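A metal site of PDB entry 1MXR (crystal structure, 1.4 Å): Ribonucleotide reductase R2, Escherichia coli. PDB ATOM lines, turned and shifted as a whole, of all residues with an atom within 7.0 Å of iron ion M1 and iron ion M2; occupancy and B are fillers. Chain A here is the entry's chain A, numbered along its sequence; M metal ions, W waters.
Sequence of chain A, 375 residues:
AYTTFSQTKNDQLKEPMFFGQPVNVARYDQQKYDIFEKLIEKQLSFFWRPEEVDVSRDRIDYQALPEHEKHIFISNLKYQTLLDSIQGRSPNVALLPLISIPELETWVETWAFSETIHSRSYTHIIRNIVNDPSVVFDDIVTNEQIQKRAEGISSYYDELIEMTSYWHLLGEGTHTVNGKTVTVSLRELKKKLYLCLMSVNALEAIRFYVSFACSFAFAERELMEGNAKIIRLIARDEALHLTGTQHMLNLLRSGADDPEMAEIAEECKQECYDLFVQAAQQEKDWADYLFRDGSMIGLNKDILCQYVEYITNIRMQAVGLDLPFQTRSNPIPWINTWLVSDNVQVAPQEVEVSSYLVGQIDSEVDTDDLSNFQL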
ATOM      1  N   GLN A  80       4.617 -12.227 -17.021  1.00  0.00           N
ATOM      2  CA  GLN A  80       4.306 -12.917 -18.285  1.00  0.00           C
ATOM      3  C   GLN A  80       2.794 -12.946 -18.465  1.00  0.00           C
ATOM      4  O   GLN A  80       2.302 -12.718 -19.592  1.00  0.00           O
ATOM      5  CB  GLN A  80       4.844 -14.367 -18.250  1.00  0.00           C
ATOM      6  CG  GLN A  80       6.395 -14.415 -18.210  1.00  0.00           C
ATOM      7  CD  GLN A  80       6.986 -15.821 -17.974  1.00  0.00           C
ATOM      8  OE1 GLN A  80       6.424 -16.644 -17.260  1.00  0.00           O
ATOM      9  NE2 GLN A  80       8.144 -16.089 -18.599  1.00  0.00           N
ATOM     10  N   LEU A  83       1.533  -9.496 -19.553  1.00  0.00           N
ATOM     11  CA  LEU A  83       1.817  -9.138 -20.942  1.00  0.00           C
ATOM     12  C   LEU A  83       0.965  -9.908 -21.915  1.00  0.00           C
ATOM     13  O   LEU A  83       0.469  -9.322 -22.920  1.00  0.00           O
ATOM     14  CB  LEU A  83       3.294  -9.371 -21.269  1.00  0.00           C
ATOM     15  CG  LEU A  83       4.344  -8.476 -20.616  1.00  0.00           C
ATOM     16  CD1 LEU A  83       5.692  -8.755 -21.216  1.00  0.00           C
ATOM     17  CD2 LEU A  83       4.017  -7.017 -20.839  1.00  0.00           C
ATOM     18  N   ASP A  84       0.738 -11.185 -21.684  1.00  0.00           N
ATOM     19  CA  ASP A  84      -0.082 -11.925 -22.623  1.00  0.00           C
ATOM     20  C   ASP A  84      -1.580 -11.744 -22.464  1.00  0.00           C
ATOM     21  O   ASP A  84      -2.340 -12.058 -23.389  1.00  0.00           O
ATOM     22  CB  ASP A  84       0.348 -13.380 -22.749  1.00  0.00           C
ATOM     23  CG  ASP A  84       1.466 -13.517 -23.790  1.00  0.00           C
ATOM     24  OD1 ASP A  84       1.864 -12.475 -24.445  1.00  0.00           O
ATOM     25  OD2 ASP A  84       1.986 -14.614 -23.954  1.00  0.00           O
ATOM     26  N   GLN A  87      -1.633  -8.957 -24.807  1.00  0.00           N
ATOM     27  CA  GLN A  87      -1.388  -9.449 -26.171  1.00  0.00           C
ATOM     28  C   GLN A  87      -2.499 -10.329 -26.719  1.00  0.00           C
ATOM     29  O   GLN A  87      -2.642 -10.491 -27.935  1.00  0.00           O
ATOM     30  CB  GLN A  87      -0.008 -10.173 -26.273  1.00  0.00           C
ATOM     31  CG  GLN A  87       1.189  -9.239 -26.165  1.00  0.00           C
ATOM     32  CD  GLN A  87       1.215  -8.335 -27.382  1.00  0.00           C
ATOM     33  OE1 GLN A  87       1.691  -8.726 -28.477  1.00  0.00           O
ATOM     34  NE2 GLN A  87       0.679  -7.155 -27.233  1.00  0.00           N
ATOM     35  N   TRP A 111      -2.126 -14.753 -34.457  1.00  0.00           N
ATOM     36  CA  TRP A 111      -1.189 -14.275 -33.459  1.00  0.00           C
ATOM     37  C   TRP A 111      -1.946 -14.035 -32.156  1.00  0.00           C
ATOM     38  O   TRP A 111      -1.583 -14.565 -31.070  1.00  0.00           O
ATOM     39  CB  TRP A 111      -0.594 -12.981 -34.019  1.00  0.00           C
ATOM     40  CG  TRP A 111       0.245 -12.129 -33.104  1.00  0.00           C
ATOM     41  CD1 TRP A 111       0.861 -12.467 -31.928  1.00  0.00           C
ATOM     42  CD2 TRP A 111       0.590 -10.778 -33.352  1.00  0.00           C
ATOM     43  NE1 TRP A 111       1.589 -11.383 -31.433  1.00  0.00           N
ATOM     44  CE2 TRP A 111       1.426 -10.340 -32.313  1.00  0.00           C
ATOM     45  CE3 TRP A 111       0.277  -9.889 -34.405  1.00  0.00           C
ATOM     46  CZ2 TRP A 111       1.958  -9.043 -32.284  1.00  0.00           C
ATOM     47  CZ3 TRP A 111       0.799  -8.600 -34.370  1.00  0.00           C
ATOM     48  CH2 TRP A 111       1.625  -8.187 -33.319  1.00  0.00           C
ATOM     49  N   SER A 114      -3.056 -17.242 -30.570  1.00  0.00           N
ATOM     50  CA  SER A 114      -1.964 -17.984 -29.942  1.00  0.00           C
ATOM     51  C   SER A 114      -1.619 -17.369 -28.583  1.00  0.00           C
ATOM     52  O   SER A 114      -1.190 -18.094 -27.653  1.00  0.00           O
ATOM     53  CB  SER A 114      -0.755 -18.040 -30.861  1.00  0.00           C
ATOM     54  OG  SER A 114      -0.034 -16.828 -30.875  1.00  0.00           O
ATOM     55  N   GLU A 115      -1.803 -16.072 -28.402  1.00  0.00           N
ATOM     56  CA  GLU A 115      -1.560 -15.445 -27.102  1.00  0.00           C
ATOM     57  C   GLU A 115      -2.579 -15.908 -26.066  1.00  0.00           C
ATOM     58  O   GLU A 115      -2.246 -16.022 -24.862  1.00  0.00           O
ATOM     59  CB  GLU A 115      -1.625 -13.920 -27.224  1.00  0.00           C
ATOM     60  CG  GLU A 115      -0.623 -13.316 -28.204  1.00  0.00           C
ATOM     61  CD  GLU A 115       0.793 -13.411 -27.747  1.00  0.00           C
ATOM     62  OE1 GLU A 115       1.069 -14.188 -26.786  1.00  0.00           O
ATOM     63  OE2 GLU A 115       1.659 -12.713 -28.304  1.00  0.00           O
ATOM     64  N   THR A 116      -3.836 -16.173 -26.460  1.00  0.00           N
ATOM     65  CA  THR A 116      -4.821 -16.668 -25.495  1.00  0.00           C
ATOM     66  C   THR A 116      -4.402 -18.069 -25.063  1.00  0.00           C
ATOM     67  O   THR A 116      -4.734 -18.450 -23.931  1.00  0.00           O
ATOM     68  CB  THR A 116      -6.298 -16.679 -26.037  1.00  0.00           C
ATOM     69  OG1 THR A 116      -6.460 -17.644 -27.094  1.00  0.00           O
ATOM     70  CG2 THR A 116      -6.679 -15.290 -26.555  1.00  0.00           C
ATOM     71  N   HIS A 118      -1.253 -18.912 -24.681  1.00  0.00           N
ATOM     72  CA  HIS A 118      -0.224 -18.630 -23.655  1.00  0.00           C
ATOM     73  C   HIS A 118      -0.892 -18.308 -22.337  1.00  0.00           C
ATOM     74  O   HIS A 118      -0.461 -18.828 -21.284  1.00  0.00           O
ATOM     75  CB  HIS A 118       0.669 -17.467 -24.104  1.00  0.00           C
ATOM     76  CG  HIS A 118       1.423 -17.805 -25.344  1.00  0.00           C
ATOM     77  ND1 HIS A 118       2.282 -16.934 -25.981  1.00  0.00           N
ATOM     78  CD2 HIS A 118       1.423 -18.934 -26.081  1.00  0.00           C
ATOM     79  CE1 HIS A 118       2.792 -17.525 -27.057  1.00  0.00           C
ATOM     80  NE2 HIS A 118       2.275 -18.744 -27.142  1.00  0.00           N
ATOM     81  N   SER A 119      -1.913 -17.455 -22.326  1.00  0.00           N
ATOM     82  CA  SER A 119      -2.625 -17.124 -21.084  1.00  0.00           C
ATOM     83  C   SER A 119      -3.188 -18.361 -20.437  1.00  0.00           C
ATOM     84  O   SER A 119      -3.091 -18.522 -19.230  1.00  0.00           O
ATOM     85  CB  SER A 119      -3.755 -16.137 -21.367  1.00  0.00           C
ATOM     86  OG  SER A 119      -3.196 -14.926 -21.874  1.00  0.00           O
ATOM     87  N   TYR A 122      -0.494 -20.154 -18.535  1.00  0.00           N
ATOM     88  CA  TYR A 122      -0.133 -19.561 -17.246  1.00  0.00           C
ATOM     89  C   TYR A 122      -1.179 -19.956 -16.199  1.00  0.00           C
ATOM     90  O   TYR A 122      -0.824 -20.225 -15.036  1.00  0.00           O
ATOM     91  CB  TYR A 122      -0.019 -18.028 -17.348  1.00  0.00           C
ATOM     92  CG  TYR A 122       0.949 -17.568 -18.379  1.00  0.00           C
ATOM     93  CD1 TYR A 122       2.218 -18.127 -18.499  1.00  0.00           C
ATOM     94  CD2 TYR A 122       0.585 -16.539 -19.273  1.00  0.00           C
ATOM     95  CE1 TYR A 122       3.111 -17.683 -19.501  1.00  0.00           C
ATOM     96  CE2 TYR A 122       1.437 -16.106 -20.209  1.00  0.00           C
ATOM     97  CZ  TYR A 122       2.692 -16.670 -20.353  1.00  0.00           C
ATOM     98  OH  TYR A 122       3.496 -16.212 -21.380  1.00  0.00           O
ATOM     99  N   LEU A 203       8.157  -5.332 -26.947  1.00  0.00           N
ATOM    100  CA  LEU A 203       7.480  -6.172 -25.973  1.00  0.00           C
ATOM    101  C   LEU A 203       7.760  -7.648 -26.175  1.00  0.00           C
ATOM    102  O   LEU A 203       8.205  -8.362 -25.239  1.00  0.00           O
ATOM    103  CB  LEU A 203       5.961  -5.924 -26.080  1.00  0.00           C
ATOM    104  CG  LEU A 203       4.984  -6.554 -25.076  1.00  0.00           C
ATOM    105  CD1 LEU A 203       3.598  -5.894 -25.199  1.00  0.00           C
ATOM    106  CD2 LEU A 203       4.834  -8.096 -25.299  1.00  0.00           C
ATOM    107  N   GLU A 204       7.526  -8.135 -27.383  1.00  0.00           N
ATOM    108  CA  GLU A 204       7.749  -9.572 -27.608  1.00  0.00           C
ATOM    109  C   GLU A 204       9.198  -9.956 -27.798  1.00  0.00           C
ATOM    110  O   GLU A 204       9.606 -11.029 -27.350  1.00  0.00           O
ATOM    111  CB  GLU A 204       6.927 -10.013 -28.795  1.00  0.00           C
ATOM    112  CG  GLU A 204       5.436  -9.842 -28.522  1.00  0.00           C
ATOM    113  CD  GLU A 204       4.560 -10.383 -29.642  1.00  0.00           C
ATOM    114  OE1 GLU A 204       4.738  -9.945 -30.812  1.00  0.00           O
ATOM    115  OE2 GLU A 204       3.694 -11.263 -29.338  1.00  0.00           O
ATOM    116  N   PHE A 208       9.705 -10.118 -23.240  1.00  0.00           N
ATOM    117  CA  PHE A 208       9.415 -11.530 -22.987  1.00  0.00           C
ATOM    118  C   PHE A 208      10.671 -12.367 -22.938  1.00  0.00           C
ATOM    119  O   PHE A 208      10.710 -13.372 -22.184  1.00  0.00           O
ATOM    120  CB  PHE A 208       8.428 -12.065 -24.021  1.00  0.00           C
ATOM    121  CG  PHE A 208       7.044 -12.249 -23.466  1.00  0.00           C
ATOM    122  CD1 PHE A 208       6.825 -13.230 -22.496  1.00  0.00           C
ATOM    123  CD2 PHE A 208       5.980 -11.431 -23.853  1.00  0.00           C
ATOM    124  CE1 PHE A 208       5.564 -13.399 -21.924  1.00  0.00           C
ATOM    125  CE2 PHE A 208       4.705 -11.598 -23.282  1.00  0.00           C
ATOM    126  CZ  PHE A 208       4.500 -12.581 -22.312  1.00  0.00           C
ATOM    127  N   PHE A 212      11.826 -15.028 -20.242  1.00  0.00           N
ATOM    128  CA  PHE A 212      12.123 -16.426 -20.542  1.00  0.00           C
ATOM    129  C   PHE A 212      13.421 -16.814 -19.836  1.00  0.00           C
ATOM    130  O   PHE A 212      13.541 -17.919 -19.299  1.00  0.00           O
ATOM    131  CB  PHE A 212      12.296 -16.676 -22.054  1.00  0.00           C
ATOM    132  CG  PHE A 212      11.050 -16.414 -22.872  1.00  0.00           C
ATOM    133  CD1 PHE A 212       9.774 -16.497 -22.325  1.00  0.00           C
ATOM    134  CD2 PHE A 212      11.185 -16.082 -24.221  1.00  0.00           C
ATOM    135  CE1 PHE A 212       8.627 -16.240 -23.125  1.00  0.00           C
ATOM    136  CE2 PHE A 212      10.036 -15.831 -25.001  1.00  0.00           C
ATOM    137  CZ  PHE A 212       8.803 -15.910 -24.438  1.00  0.00           C
ATOM    138  N   ILE A 234       6.015 -21.541 -25.640  1.00  0.00           N
ATOM    139  CA  ILE A 234       5.692 -20.110 -25.745  1.00  0.00           C
ATOM    140  C   ILE A 234       6.791 -19.355 -26.504  1.00  0.00           C
ATOM    141  O   ILE A 234       6.490 -18.531 -27.419  1.00  0.00           O
ATOM    142  CB  ILE A 234       5.458 -19.487 -24.345  1.00  0.00           C
ATOM    143  CG1 ILE A 234       4.137 -20.018 -23.775  1.00  0.00           C
ATOM    144  CG2 ILE A 234       5.456 -17.917 -24.445  1.00  0.00           C
ATOM    145  CD1 ILE A 234       3.850 -19.506 -22.365  1.00  0.00           C
ATOM    146  N   ASP A 237       6.637 -19.809 -30.177  1.00  0.00           N
ATOM    147  CA  ASP A 237       5.584 -18.939 -30.778  1.00  0.00           C
ATOM    148  C   ASP A 237       6.056 -17.481 -30.797  1.00  0.00           C
ATOM    149  O   ASP A 237       5.861 -16.797 -31.803  1.00  0.00           O
ATOM    150  CB  ASP A 237       4.305 -18.997 -29.937  1.00  0.00           C
ATOM    151  CG  ASP A 237       3.595 -20.352 -29.992  1.00  0.00           C
ATOM    152  OD1 ASP A 237       3.820 -21.093 -30.967  1.00  0.00           O
ATOM    153  OD2 ASP A 237       2.814 -20.583 -29.055  1.00  0.00           O
ATOM    154  N   GLU A 238       6.651 -17.014 -29.708  1.00  0.00           N
ATOM    155  CA  GLU A 238       7.098 -15.638 -29.639  1.00  0.00           C
ATOM    156  C   GLU A 238       8.074 -15.297 -30.743  1.00  0.00           C
ATOM    157  O   GLU A 238       8.088 -14.151 -31.273  1.00  0.00           O
ATOM    158  CB  GLU A 238       7.773 -15.371 -28.293  1.00  0.00           C
ATOM    159  CG  GLU A 238       7.900 -13.910 -27.983  1.00  0.00           C
ATOM    160  CD  GLU A 238       6.562 -13.293 -27.596  1.00  0.00           C
ATOM    161  OE1 GLU A 238       6.317 -13.107 -26.410  1.00  0.00           O
ATOM    162  OE2 GLU A 238       5.726 -12.987 -28.475  1.00  0.00           O
ATOM    163  N   ALA A 239       8.890 -16.265 -31.142  1.00  0.00           N
ATOM    164  CA  ALA A 239       9.852 -16.006 -32.222  1.00  0.00           C
ATOM    165  C   ALA A 239       9.076 -15.676 -33.512  1.00  0.00           C
ATOM    166  O   ALA A 239       9.502 -14.836 -34.309  1.00  0.00           O
ATOM    167  CB  ALA A 239      10.777 -17.240 -32.426  1.00  0.00           C
ATOM    168  N   HIS A 241       6.042 -14.320 -33.549  1.00  0.00           N
ATOM    169  CA  HIS A 241       5.392 -13.015 -33.326  1.00  0.00           C
ATOM    170  C   HIS A 241       6.332 -11.860 -33.603  1.00  0.00           C
ATOM    171  O   HIS A 241       5.973 -10.929 -34.307  1.00  0.00           O
ATOM    172  CB  HIS A 241       4.834 -12.892 -31.916  1.00  0.00           C
ATOM    173  CG  HIS A 241       3.888 -14.006 -31.562  1.00  0.00           C
ATOM    174  ND1 HIS A 241       3.386 -14.181 -30.291  1.00  0.00           N
ATOM    175  CD2 HIS A 241       3.334 -14.971 -32.329  1.00  0.00           C
ATOM    176  CE1 HIS A 241       2.551 -15.204 -30.299  1.00  0.00           C
ATOM    177  NE2 HIS A 241       2.508 -15.705 -31.514  1.00  0.00           N
ATOM    178  N   LEU A 242       7.551 -11.909 -33.075  1.00  0.00           N
ATOM    179  CA  LEU A 242       8.489 -10.813 -33.330  1.00  0.00           C
ATOM    180  C   LEU A 242       8.964 -10.834 -34.787  1.00  0.00           C
ATOM    181  O   LEU A 242       9.291  -9.774 -35.380  1.00  0.00           O
ATOM    182  CB  LEU A 242       9.657 -10.901 -32.311  1.00  0.00           C
ATOM    183  CG  LEU A 242      10.663 -12.069 -32.516  1.00  0.00           C
ATOM    184  CD1 LEU A 242      11.834 -11.709 -33.446  1.00  0.00           C
ATOM    185  CD2 LEU A 242      11.216 -12.525 -31.132  1.00  0.00           C
HETATM  186 FE    FE M   1       2.698 -14.856 -25.792  1.00  0.00          FE
HETATM  187 FE    FE M   2       3.677 -12.994 -28.435  1.00  0.00          FE
HETATM  188  O   HOH W   1       3.732 -14.635 -27.409  1.00  0.00           O
HETATM  189  O   HOH W   2       4.737 -14.795 -24.722  1.00  0.00           O
HETATM  190  O   HOH W   3       3.878 -11.926 -26.405  1.00  0.00           O
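Iron ion M1 is bound by water W1, OD2 of Asp 84, OE1 of Glu 115, ND1 of His 118 and water W2. Iron ion M1 has five donor atoms within binding distance.
Iron ion M2 is bound by water W1 (1.9 Å), the side-chain carboxylate of Glu 204 (2.0 Å), the side-chain carboxylate of Glu 115 (2.0 Å), the side-chain carboxylate of Glu 238 (2.0 Å), a ring nitrogen (ND1) of His 241 (2.2 Å) and water W3 (2.3 Å).
Water W3 lies within hydrogen-bond range of the side-chain carboxylate (OE1) of Glu 238 (2.7 Å) and the side-chain carboxylate (OD1) of Asp 84 (2.9 Å).
The backbone carbonyl oxygen (O) of Trp 111 sits at hydrogen-bond distance from the side-chain hydroxyl (OG) of Ser 114 (2.7 Å). OE2 of Glu 115 sits close to NE1 of Trp 111. OD2 of Asp 237 lies within hydrogen-bond range of NE2 of His 118 (2.7 Å). OD2 of Asp 84 lies close to OH of Tyr 122, at 3.4 Å. The side-chain hydroxyl (OG) of Ser 119 sits at hydrogen-bond distance from the backbone carbonyl oxygen (O) of Glu 115, 3.3 Å away. O of Asp 84 sits at hydrogen-bond distance from OG of Ser 119 (3.4 Å). The indole nitrogen (NE1) of Trp 111 lies close to the side-chain carboxylate (OE2) of Glu 204. A ring nitrogen (NE2) of His 241 sits at hydrogen-bond distance from the side-chain hydroxyl (OG) of Ser 114, 2.9 Å away.
Merely in contact with iron ion M2: Trp 111. Of the 21 residues printed, 5 come within 4 Å of iron ion M2. The nearest printed residue that does not touch iron ion M2 is Asp 84 (4.4 Å).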
